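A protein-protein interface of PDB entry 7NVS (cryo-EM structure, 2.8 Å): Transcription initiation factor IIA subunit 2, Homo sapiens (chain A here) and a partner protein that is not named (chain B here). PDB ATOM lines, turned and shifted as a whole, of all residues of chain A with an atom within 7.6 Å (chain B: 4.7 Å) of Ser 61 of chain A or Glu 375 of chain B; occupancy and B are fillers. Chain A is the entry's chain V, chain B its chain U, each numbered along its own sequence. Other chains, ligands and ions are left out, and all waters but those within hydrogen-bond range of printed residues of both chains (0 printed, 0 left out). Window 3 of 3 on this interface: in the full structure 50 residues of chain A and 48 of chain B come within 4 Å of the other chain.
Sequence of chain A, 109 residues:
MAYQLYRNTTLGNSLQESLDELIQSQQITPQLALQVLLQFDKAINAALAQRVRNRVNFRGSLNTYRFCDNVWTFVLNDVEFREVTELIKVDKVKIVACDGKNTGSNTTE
OG of Ser 61 of chain A is in hydrogen-bond range of O of Glu 375 of chain B (3.5 Å).
The backbone carbonyl oxygen (O) of Glu 375 of chain B lies within hydrogen-bond range of the backbone NH (N) of Leu 62 of chain A (2.9 Å).
The side-chain carboxylate of Asp 373 of chain B is in salt-bridge range of the guanidinium group of Arg 59 of chain A (3.8 Å).
O of Asp 373 of chain B sits close to O of Gly 60 of chain A, at 3.5 Å.
The backbone NH (N) of Trp 376 of chain B is in hydrogen-bond range of the backbone carbonyl oxygen (O) of Asn 347 of chain B (3.3 Å).
The backbone carbonyl oxygen (O) of Val 93 of chain A lies within hydrogen-bond range of the backbone NH (N) of Leu 76 of chain A (2.8 Å).
The side-chain carboxylate of Glu 375 of chain B sits close to the side-chain amide oxygen of Asn 347 of chain B (3.5 Å).
The backbone NH (N) of Asn 63 of chain A lies within hydrogen-bond range of the backbone carbonyl oxygen (O) of Val 75 of chain A, at 2.9 Å.
The backbone NH (N) of Asn 77 of chain A is in hydrogen-bond range of the backbone carbonyl oxygen (O) of Ser 61 of chain A (2.6 Å).
The backbone carbonyl oxygen (O) of Arg 59 of chain A sits at hydrogen-bond distance from the backbone NH (N) of Glu 80 of chain A, at 2.5 Å.
Among the printed residues, pairs that only touch across the chains: Gly 60 of chain A with Ala 374 of chain B, Leu 62 of chain A with Trp 376 of chain B, Asn 63 of chain A with Trp 376 of chain B, Leu 76 of chain A with Ala 374 of chain B, Leu 62 of chain A with Ala 374 of chain B and Gly 60 of chain A with Glu 375 of chain B.
Of the printed residues of chain B, Gly 60 of chain A touches Asp 373 (3.5 Å), Ala 374 (3.3 Å) and Glu 375 (3.8 Å).
Ser 61 of chain A touches just one residue of chain B: Glu 375 (3.5 Å).
Of the printed residues of chain B, Asn 63 of chain A touches Trp 376.
Printed residues of chain B within 4 Å of Leu 76 of chain A: Ala 374.
Asp 78 of chain A touches none of the printed residues of chain B.
Of the printed residues of chain A, Ala 374 of chain B touches Gly 60 (3.3 Å), Leu 62 (3.8 Å) and Leu 76 (3.6 Å).
Of chain A, only Gly 60 (3.8 Å), Ser 61 (3.5 Å) and Leu 62 (2.9 Å) come within 4 Å of Glu 375 of chain B.
Printed residues of chain A within 4 Å of Trp 376 of chain B: Leu 62 (3.3 Å) and Asn 63 (3.5 Å).
Printed residues of chain A that touch a printed residue of chain B: Arg 59, Gly 60, Ser 61, Leu 62, Asn 63 and Leu 76.
Hydrophobic or aromatic side chains of chain B that line the printed part of chain A: Ala 374 and Trp 376.
Among the printed residues, 10 pairs touch across the chains.
Among the printed residues, Asp or Glu carboxylates within 4 Å of a Lys or Arg side-chain nitrogen of the other chain: Arg 59 of chain A with Asp 373 of chain B (3.8 Å).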
ATOM      1  N   ARG A  59      29.170  10.268 -18.791  1.00  0.00           N
ATOM      2  CA  ARG A  59      28.651  10.949 -19.971  1.00  0.00           C
ATOM      3  C   ARG A  59      27.137  10.800 -19.989  1.00  0.00           C
ATOM      4  O   ARG A  59      26.603   9.839 -19.429  1.00  0.00           O
ATOM      5  CB  ARG A  59      29.251  10.377 -21.262  1.00  0.00           C
ATOM      6  CG  ARG A  59      30.768  10.441 -21.339  1.00  0.00           C
ATOM      7  CD  ARG A  59      31.247  11.783 -21.873  1.00  0.00           C
ATOM      8  NE  ARG A  59      32.638  11.723 -22.318  1.00  0.00           N
ATOM      9  CZ  ARG A  59      33.146  12.438 -23.319  1.00  0.00           C
ATOM     10  NH1 ARG A  59      32.389  13.293 -23.996  1.00  0.00           N
ATOM     11  NH2 ARG A  59      34.425  12.302 -23.641  1.00  0.00           N
ATOM     12  N   GLY A  60      26.454  11.746 -20.628  1.00  0.00           N
ATOM     13  CA  GLY A  60      25.006  11.706 -20.681  1.00  0.00           C
ATOM     14  C   GLY A  60      24.456  12.838 -21.520  1.00  0.00           C
ATOM     15  O   GLY A  60      25.195  13.573 -22.177  1.00  0.00           O
ATOM     16  N   SER A  61      23.132  12.961 -21.493  1.00  0.00           N
ATOM     17  CA  SER A  61      22.409  14.002 -22.214  1.00  0.00           C
ATOM     18  C   SER A  61      21.736  14.932 -21.215  1.00  0.00           C
ATOM     19  O   SER A  61      21.113  14.472 -20.252  1.00  0.00           O
ATOM     20  CB  SER A  61      21.368  13.391 -23.155  1.00  0.00           C
ATOM     21  OG  SER A  61      20.618  14.400 -23.809  1.00  0.00           O
ATOM     22  N   LEU A  62      21.861  16.238 -21.445  1.00  0.00           N
ATOM     23  CA  LEU A  62      21.294  17.231 -20.543  1.00  0.00           C
ATOM     24  C   LEU A  62      19.871  17.576 -20.965  1.00  0.00           C
ATOM     25  O   LEU A  62      19.598  17.792 -22.150  1.00  0.00           O
ATOM     26  CB  LEU A  62      22.161  18.490 -20.525  1.00  0.00           C
ATOM     27  CG  LEU A  62      21.926  19.461 -19.364  1.00  0.00           C
ATOM     28  CD1 LEU A  62      23.224  20.157 -18.989  1.00  0.00           C
ATOM     29  CD2 LEU A  62      20.857  20.486 -19.707  1.00  0.00           C
ATOM     30  N   ASN A  63      18.965  17.627 -19.989  1.00  0.00           N
ATOM     31  CA  ASN A  63      17.563  17.954 -20.226  1.00  0.00           C
ATOM     32  C   ASN A  63      17.149  19.285 -19.611  1.00  0.00           C
ATOM     33  O   ASN A  63      16.352  20.014 -20.210  1.00  0.00           O
ATOM     34  CB  ASN A  63      16.664  16.842 -19.675  1.00  0.00           C
ATOM     35  CG  ASN A  63      15.191  17.126 -19.886  1.00  0.00           C
ATOM     36  OD1 ASN A  63      14.796  17.708 -20.896  1.00  0.00           O
ATOM     37  ND2 ASN A  63      14.367  16.712 -18.930  1.00  0.00           N
ATOM     38  N   THR A  64      17.668  19.620 -18.432  1.00  0.00           N
ATOM     39  CA  THR A  64      17.303  20.862 -17.766  1.00  0.00           C
ATOM     40  C   THR A  64      18.463  21.307 -16.886  1.00  0.00           C
ATOM     41  O   THR A  64      19.225  20.486 -16.369  1.00  0.00           O
ATOM     42  CB  THR A  64      16.027  20.698 -16.931  1.00  0.00           C
ATOM     43  OG1 THR A  64      14.929  20.361 -17.790  1.00  0.00           O
ATOM     44  CG2 THR A  64      15.704  21.981 -16.179  1.00  0.00           C
ATOM     45  N   VAL A  75      19.938  18.462 -14.701  1.00  0.00           N
ATOM     46  CA  VAL A  75      19.101  17.271 -14.815  1.00  0.00           C
ATOM     47  C   VAL A  75      19.527  16.571 -16.099  1.00  0.00           C
ATOM     48  O   VAL A  75      19.257  17.061 -17.201  1.00  0.00           O
ATOM     49  CB  VAL A  75      17.605  17.603 -14.836  1.00  0.00           C
ATOM     50  CG1 VAL A  75      16.785  16.347 -15.104  1.00  0.00           C
ATOM     51  CG2 VAL A  75      17.185  18.249 -13.523  1.00  0.00           C
ATOM     52  N   LEU A  76      20.191  15.427 -15.963  1.00  0.00           N
ATOM     53  CA  LEU A  76      20.709  14.681 -17.101  1.00  0.00           C
ATOM     54  C   LEU A  76      19.869  13.432 -17.333  1.00  0.00           C
ATOM     55  O   LEU A  76      19.338  12.842 -16.387  1.00  0.00           O
ATOM     56  CB  LEU A  76      22.168  14.289 -16.874  1.00  0.00           C
ATOM     57  CG  LEU A  76      23.164  15.434 -16.678  1.00  0.00           C
ATOM     58  CD1 LEU A  76      24.503  14.894 -16.201  1.00  0.00           C
ATOM     59  CD2 LEU A  76      23.334  16.245 -17.953  1.00  0.00           C
ATOM     60  N   ASN A  77      19.753  13.035 -18.598  1.00  0.00           N
ATOM     61  CA  ASN A  77      19.015  11.845 -18.994  1.00  0.00           C
ATOM     62  C   ASN A  77      19.933  10.916 -19.775  1.00  0.00           C
ATOM     63  O   ASN A  77      20.754  11.370 -20.579  1.00  0.00           O
ATOM     64  CB  ASN A  77      17.792  12.208 -19.844  1.00  0.00           C
ATOM     65  CG  ASN A  77      16.731  12.947 -19.052  1.00  0.00           C
ATOM     66  OD1 ASN A  77      17.035  13.650 -18.087  1.00  0.00           O
ATOM     67  ND2 ASN A  77      15.476  12.791 -19.456  1.00  0.00           N
ATOM     68  N   ASP A  78      19.789   9.612 -19.535  1.00  0.00           N
ATOM     69  CA  ASP A  78      20.606   8.595 -20.193  1.00  0.00           C
ATOM     70  C   ASP A  78      22.092   8.845 -19.931  1.00  0.00           C
ATOM     71  O   ASP A  78      22.886   9.083 -20.843  1.00  0.00           O
ATOM     72  CB  ASP A  78      20.309   8.549 -21.696  1.00  0.00           C
ATOM     73  CG  ASP A  78      18.883   8.135 -21.997  1.00  0.00           C
ATOM     74  OD1 ASP A  78      18.297   7.384 -21.189  1.00  0.00           O
ATOM     75  OD2 ASP A  78      18.346   8.563 -23.041  1.00  0.00           O
ATOM     76  N   VAL A  79      22.456   8.785 -18.653  1.00  0.00           N
ATOM     77  CA  VAL A  79      23.815   9.058 -18.203  1.00  0.00           C
ATOM     78  C   VAL A  79      24.545   7.738 -18.007  1.00  0.00           C
ATOM     79  O   VAL A  79      24.028   6.816 -17.364  1.00  0.00           O
ATOM     80  CB  VAL A  79      23.817   9.882 -16.901  1.00  0.00           C
ATOM     81  CG1 VAL A  79      25.243  10.188 -16.462  1.00  0.00           C
ATOM     82  CG2 VAL A  79      23.023  11.164 -17.084  1.00  0.00           C
ATOM     83  N   GLU A  80      25.750   7.646 -18.566  1.00  0.00           N
ATOM     84  CA  GLU A  80      26.601   6.471 -18.424  1.00  0.00           C
ATOM     85  C   GLU A  80      27.814   6.858 -17.593  1.00  0.00           C
ATOM     86  O   GLU A  80      28.622   7.688 -18.021  1.00  0.00           O
ATOM     87  CB  GLU A  80      27.029   5.931 -19.795  1.00  0.00           C
ATOM     88  CG  GLU A  80      28.229   4.991 -19.764  1.00  0.00           C
ATOM     89  CD  GLU A  80      28.630   4.518 -21.147  1.00  0.00           C
ATOM     90  OE1 GLU A  80      28.720   5.363 -22.062  1.00  0.00           O
ATOM     91  OE2 GLU A  80      28.861   3.302 -21.319  1.00  0.00           O
ATOM     92  N   ASP A  91      18.970   5.976 -16.086  1.00  0.00           N
ATOM     93  CA  ASP A  91      18.084   6.641 -17.036  1.00  0.00           C
ATOM     94  C   ASP A  91      18.076   8.150 -16.825  1.00  0.00           C
ATOM     95  O   ASP A  91      18.178   8.922 -17.785  1.00  0.00           O
ATOM     96  CB  ASP A  91      16.670   6.073 -16.915  1.00  0.00           C
ATOM     97  CG  ASP A  91      15.751   6.553 -18.022  1.00  0.00           C
ATOM     98  OD1 ASP A  91      15.441   7.763 -18.057  1.00  0.00           O
ATOM     99  OD2 ASP A  91      15.340   5.721 -18.857  1.00  0.00           O
ATOM    100  N   LYS A  92      17.950   8.591 -15.573  1.00  0.00           N
ATOM    101  CA  LYS A  92      17.889  10.010 -15.256  1.00  0.00           C
ATOM    102  C   LYS A  92      18.634  10.273 -13.957  1.00  0.00           C
ATOM    103  O   LYS A  92      18.649   9.428 -13.058  1.00  0.00           O
ATOM    104  CB  LYS A  92      16.437  10.492 -15.132  1.00  0.00           C
ATOM    105  CG  LYS A  92      16.299  11.985 -14.876  1.00  0.00           C
ATOM    106  CD  LYS A  92      14.890  12.480 -15.172  1.00  0.00           C
ATOM    107  CE  LYS A  92      13.892  12.002 -14.128  1.00  0.00           C
ATOM    108  NZ  LYS A  92      14.008  12.764 -12.853  1.00  0.00           N
ATOM    109  N   VAL A  93      19.249  11.452 -13.864  1.00  0.00           N
ATOM    110  CA  VAL A  93      19.999  11.857 -12.683  1.00  0.00           C
ATOM    111  C   VAL A  93      19.876  13.364 -12.512  1.00  0.00           C
ATOM    112  O   VAL A  93      19.839  14.119 -13.489  1.00  0.00           O
ATOM    113  CB  VAL A  93      21.486  11.447 -12.774  1.00  0.00           C
ATOM    114  CG1 VAL A  93      22.290  12.088 -11.650  1.00  0.00           C
ATOM    115  CG2 VAL A  93      21.622   9.936 -12.735  1.00  0.00           C
ATOM    116  N   ASN B 347      26.687  24.184 -27.725  1.00  0.00           N
ATOM    117  CA  ASN B 347      25.973  22.917 -27.850  1.00  0.00           C
ATOM    118  C   ASN B 347      26.051  22.065 -26.590  1.00  0.00           C
ATOM    119  O   ASN B 347      25.067  21.428 -26.202  1.00  0.00           O
ATOM    120  CB  ASN B 347      26.513  22.129 -29.045  1.00  0.00           C
ATOM    121  CG  ASN B 347      25.507  21.132 -29.588  1.00  0.00           C
ATOM    122  OD1 ASN B 347      24.421  20.964 -29.032  1.00  0.00           O
ATOM    123  ND2 ASN B 347      25.861  20.470 -30.682  1.00  0.00           N
ATOM    124  N   LYS B 348      27.215  22.053 -25.944  1.00  0.00           N
ATOM    125  CA  LYS B 348      27.559  21.032 -24.968  1.00  0.00           C
ATOM    126  C   LYS B 348      27.952  21.659 -23.639  1.00  0.00           C
ATOM    127  O   LYS B 348      28.690  22.646 -23.589  1.00  0.00           O
ATOM    128  CB  LYS B 348      28.716  20.164 -25.475  1.00  0.00           C
ATOM    129  CG  LYS B 348      28.452  19.478 -26.809  1.00  0.00           C
ATOM    130  CD  LYS B 348      27.713  18.158 -26.650  1.00  0.00           C
ATOM    131  CE  LYS B 348      28.318  17.086 -27.542  1.00  0.00           C
ATOM    132  NZ  LYS B 348      27.372  15.965 -27.796  1.00  0.00           N
ATOM    133  N   ASP B 373      30.609  15.434 -19.896  1.00  0.00           N
ATOM    134  CA  ASP B 373      30.201  16.175 -21.079  1.00  0.00           C
ATOM    135  C   ASP B 373      28.765  15.805 -21.418  1.00  0.00           C
ATOM    136  O   ASP B 373      28.425  14.618 -21.477  1.00  0.00           O
ATOM    137  CB  ASP B 373      31.123  15.875 -22.265  1.00  0.00           C
ATOM    138  CG  ASP B 373      31.161  17.003 -23.275  1.00  0.00           C
ATOM    139  OD1 ASP B 373      30.201  17.801 -23.314  1.00  0.00           O
ATOM    140  OD2 ASP B 373      32.152  17.093 -24.031  1.00  0.00           O
ATOM    141  N   ALA B 374      27.929  16.817 -21.638  1.00  0.00           N
ATOM    142  CA  ALA B 374      26.517  16.606 -21.920  1.00  0.00           C
ATOM    143  C   ALA B 374      26.093  17.497 -23.077  1.00  0.00           C
ATOM    144  O   ALA B 374      26.710  18.528 -23.356  1.00  0.00           O
ATOM    145  CB  ALA B 374      25.647  16.888 -20.689  1.00  0.00           C
ATOM    146  N   GLU B 375      25.023  17.081 -23.752  1.00  0.00           N
ATOM    147  CA  GLU B 375      24.467  17.801 -24.889  1.00  0.00           C
ATOM    148  C   GLU B 375      23.053  18.249 -24.552  1.00  0.00           C
ATOM    149  O   GLU B 375      22.256  17.460 -24.035  1.00  0.00           O
ATOM    150  CB  GLU B 375      24.461  16.927 -26.145  1.00  0.00           C
ATOM    151  CG  GLU B 375      24.036  17.660 -27.410  1.00  0.00           C
ATOM    152  CD  GLU B 375      22.534  17.646 -27.626  1.00  0.00           C
ATOM    153  OE1 GLU B 375      21.877  16.664 -27.217  1.00  0.00           O
ATOM    154  OE2 GLU B 375      22.008  18.619 -28.206  1.00  0.00           O
ATOM    155  N   TRP B 376      22.749  19.509 -24.845  1.00  0.00           N
ATOM    156  CA  TRP B 376      21.420  20.058 -24.595  1.00  0.00           C
ATOM    157  C   TRP B 376      20.715  20.382 -25.907  1.00  0.00           C
ATOM    158  O   TRP B 376      19.676  19.801 -26.225  1.00  0.00           O
ATOM    159  CB  TRP B 376      21.513  21.312 -23.725  1.00  0.00           C
ATOM    160  CG  TRP B 376      20.176  21.870 -23.340  1.00  0.00           C
ATOM    161  CD1 TRP B 376      19.262  21.303 -22.503  1.00  0.00           C
ATOM    162  CD2 TRP B 376      19.605  23.110 -23.776  1.00  0.00           C
ATOM    163  NE1 TRP B 376      18.157  22.110 -22.390  1.00  0.00           N
ATOM    164  CE2 TRP B 376      18.342  23.227 -23.163  1.00  0.00           C
ATOM    165  CE3 TRP B 376      20.039  24.132 -24.627  1.00  0.00           C
ATOM    166  CZ2 TRP B 376      17.509  24.322 -23.372  1.00  0.00           C
ATOM    167  CZ3 TRP B 376      19.210  25.220 -24.832  1.00  0.00           C
ATOM    168  CH2 TRP B 376      17.959  25.306 -24.208  1.00  0.00           C
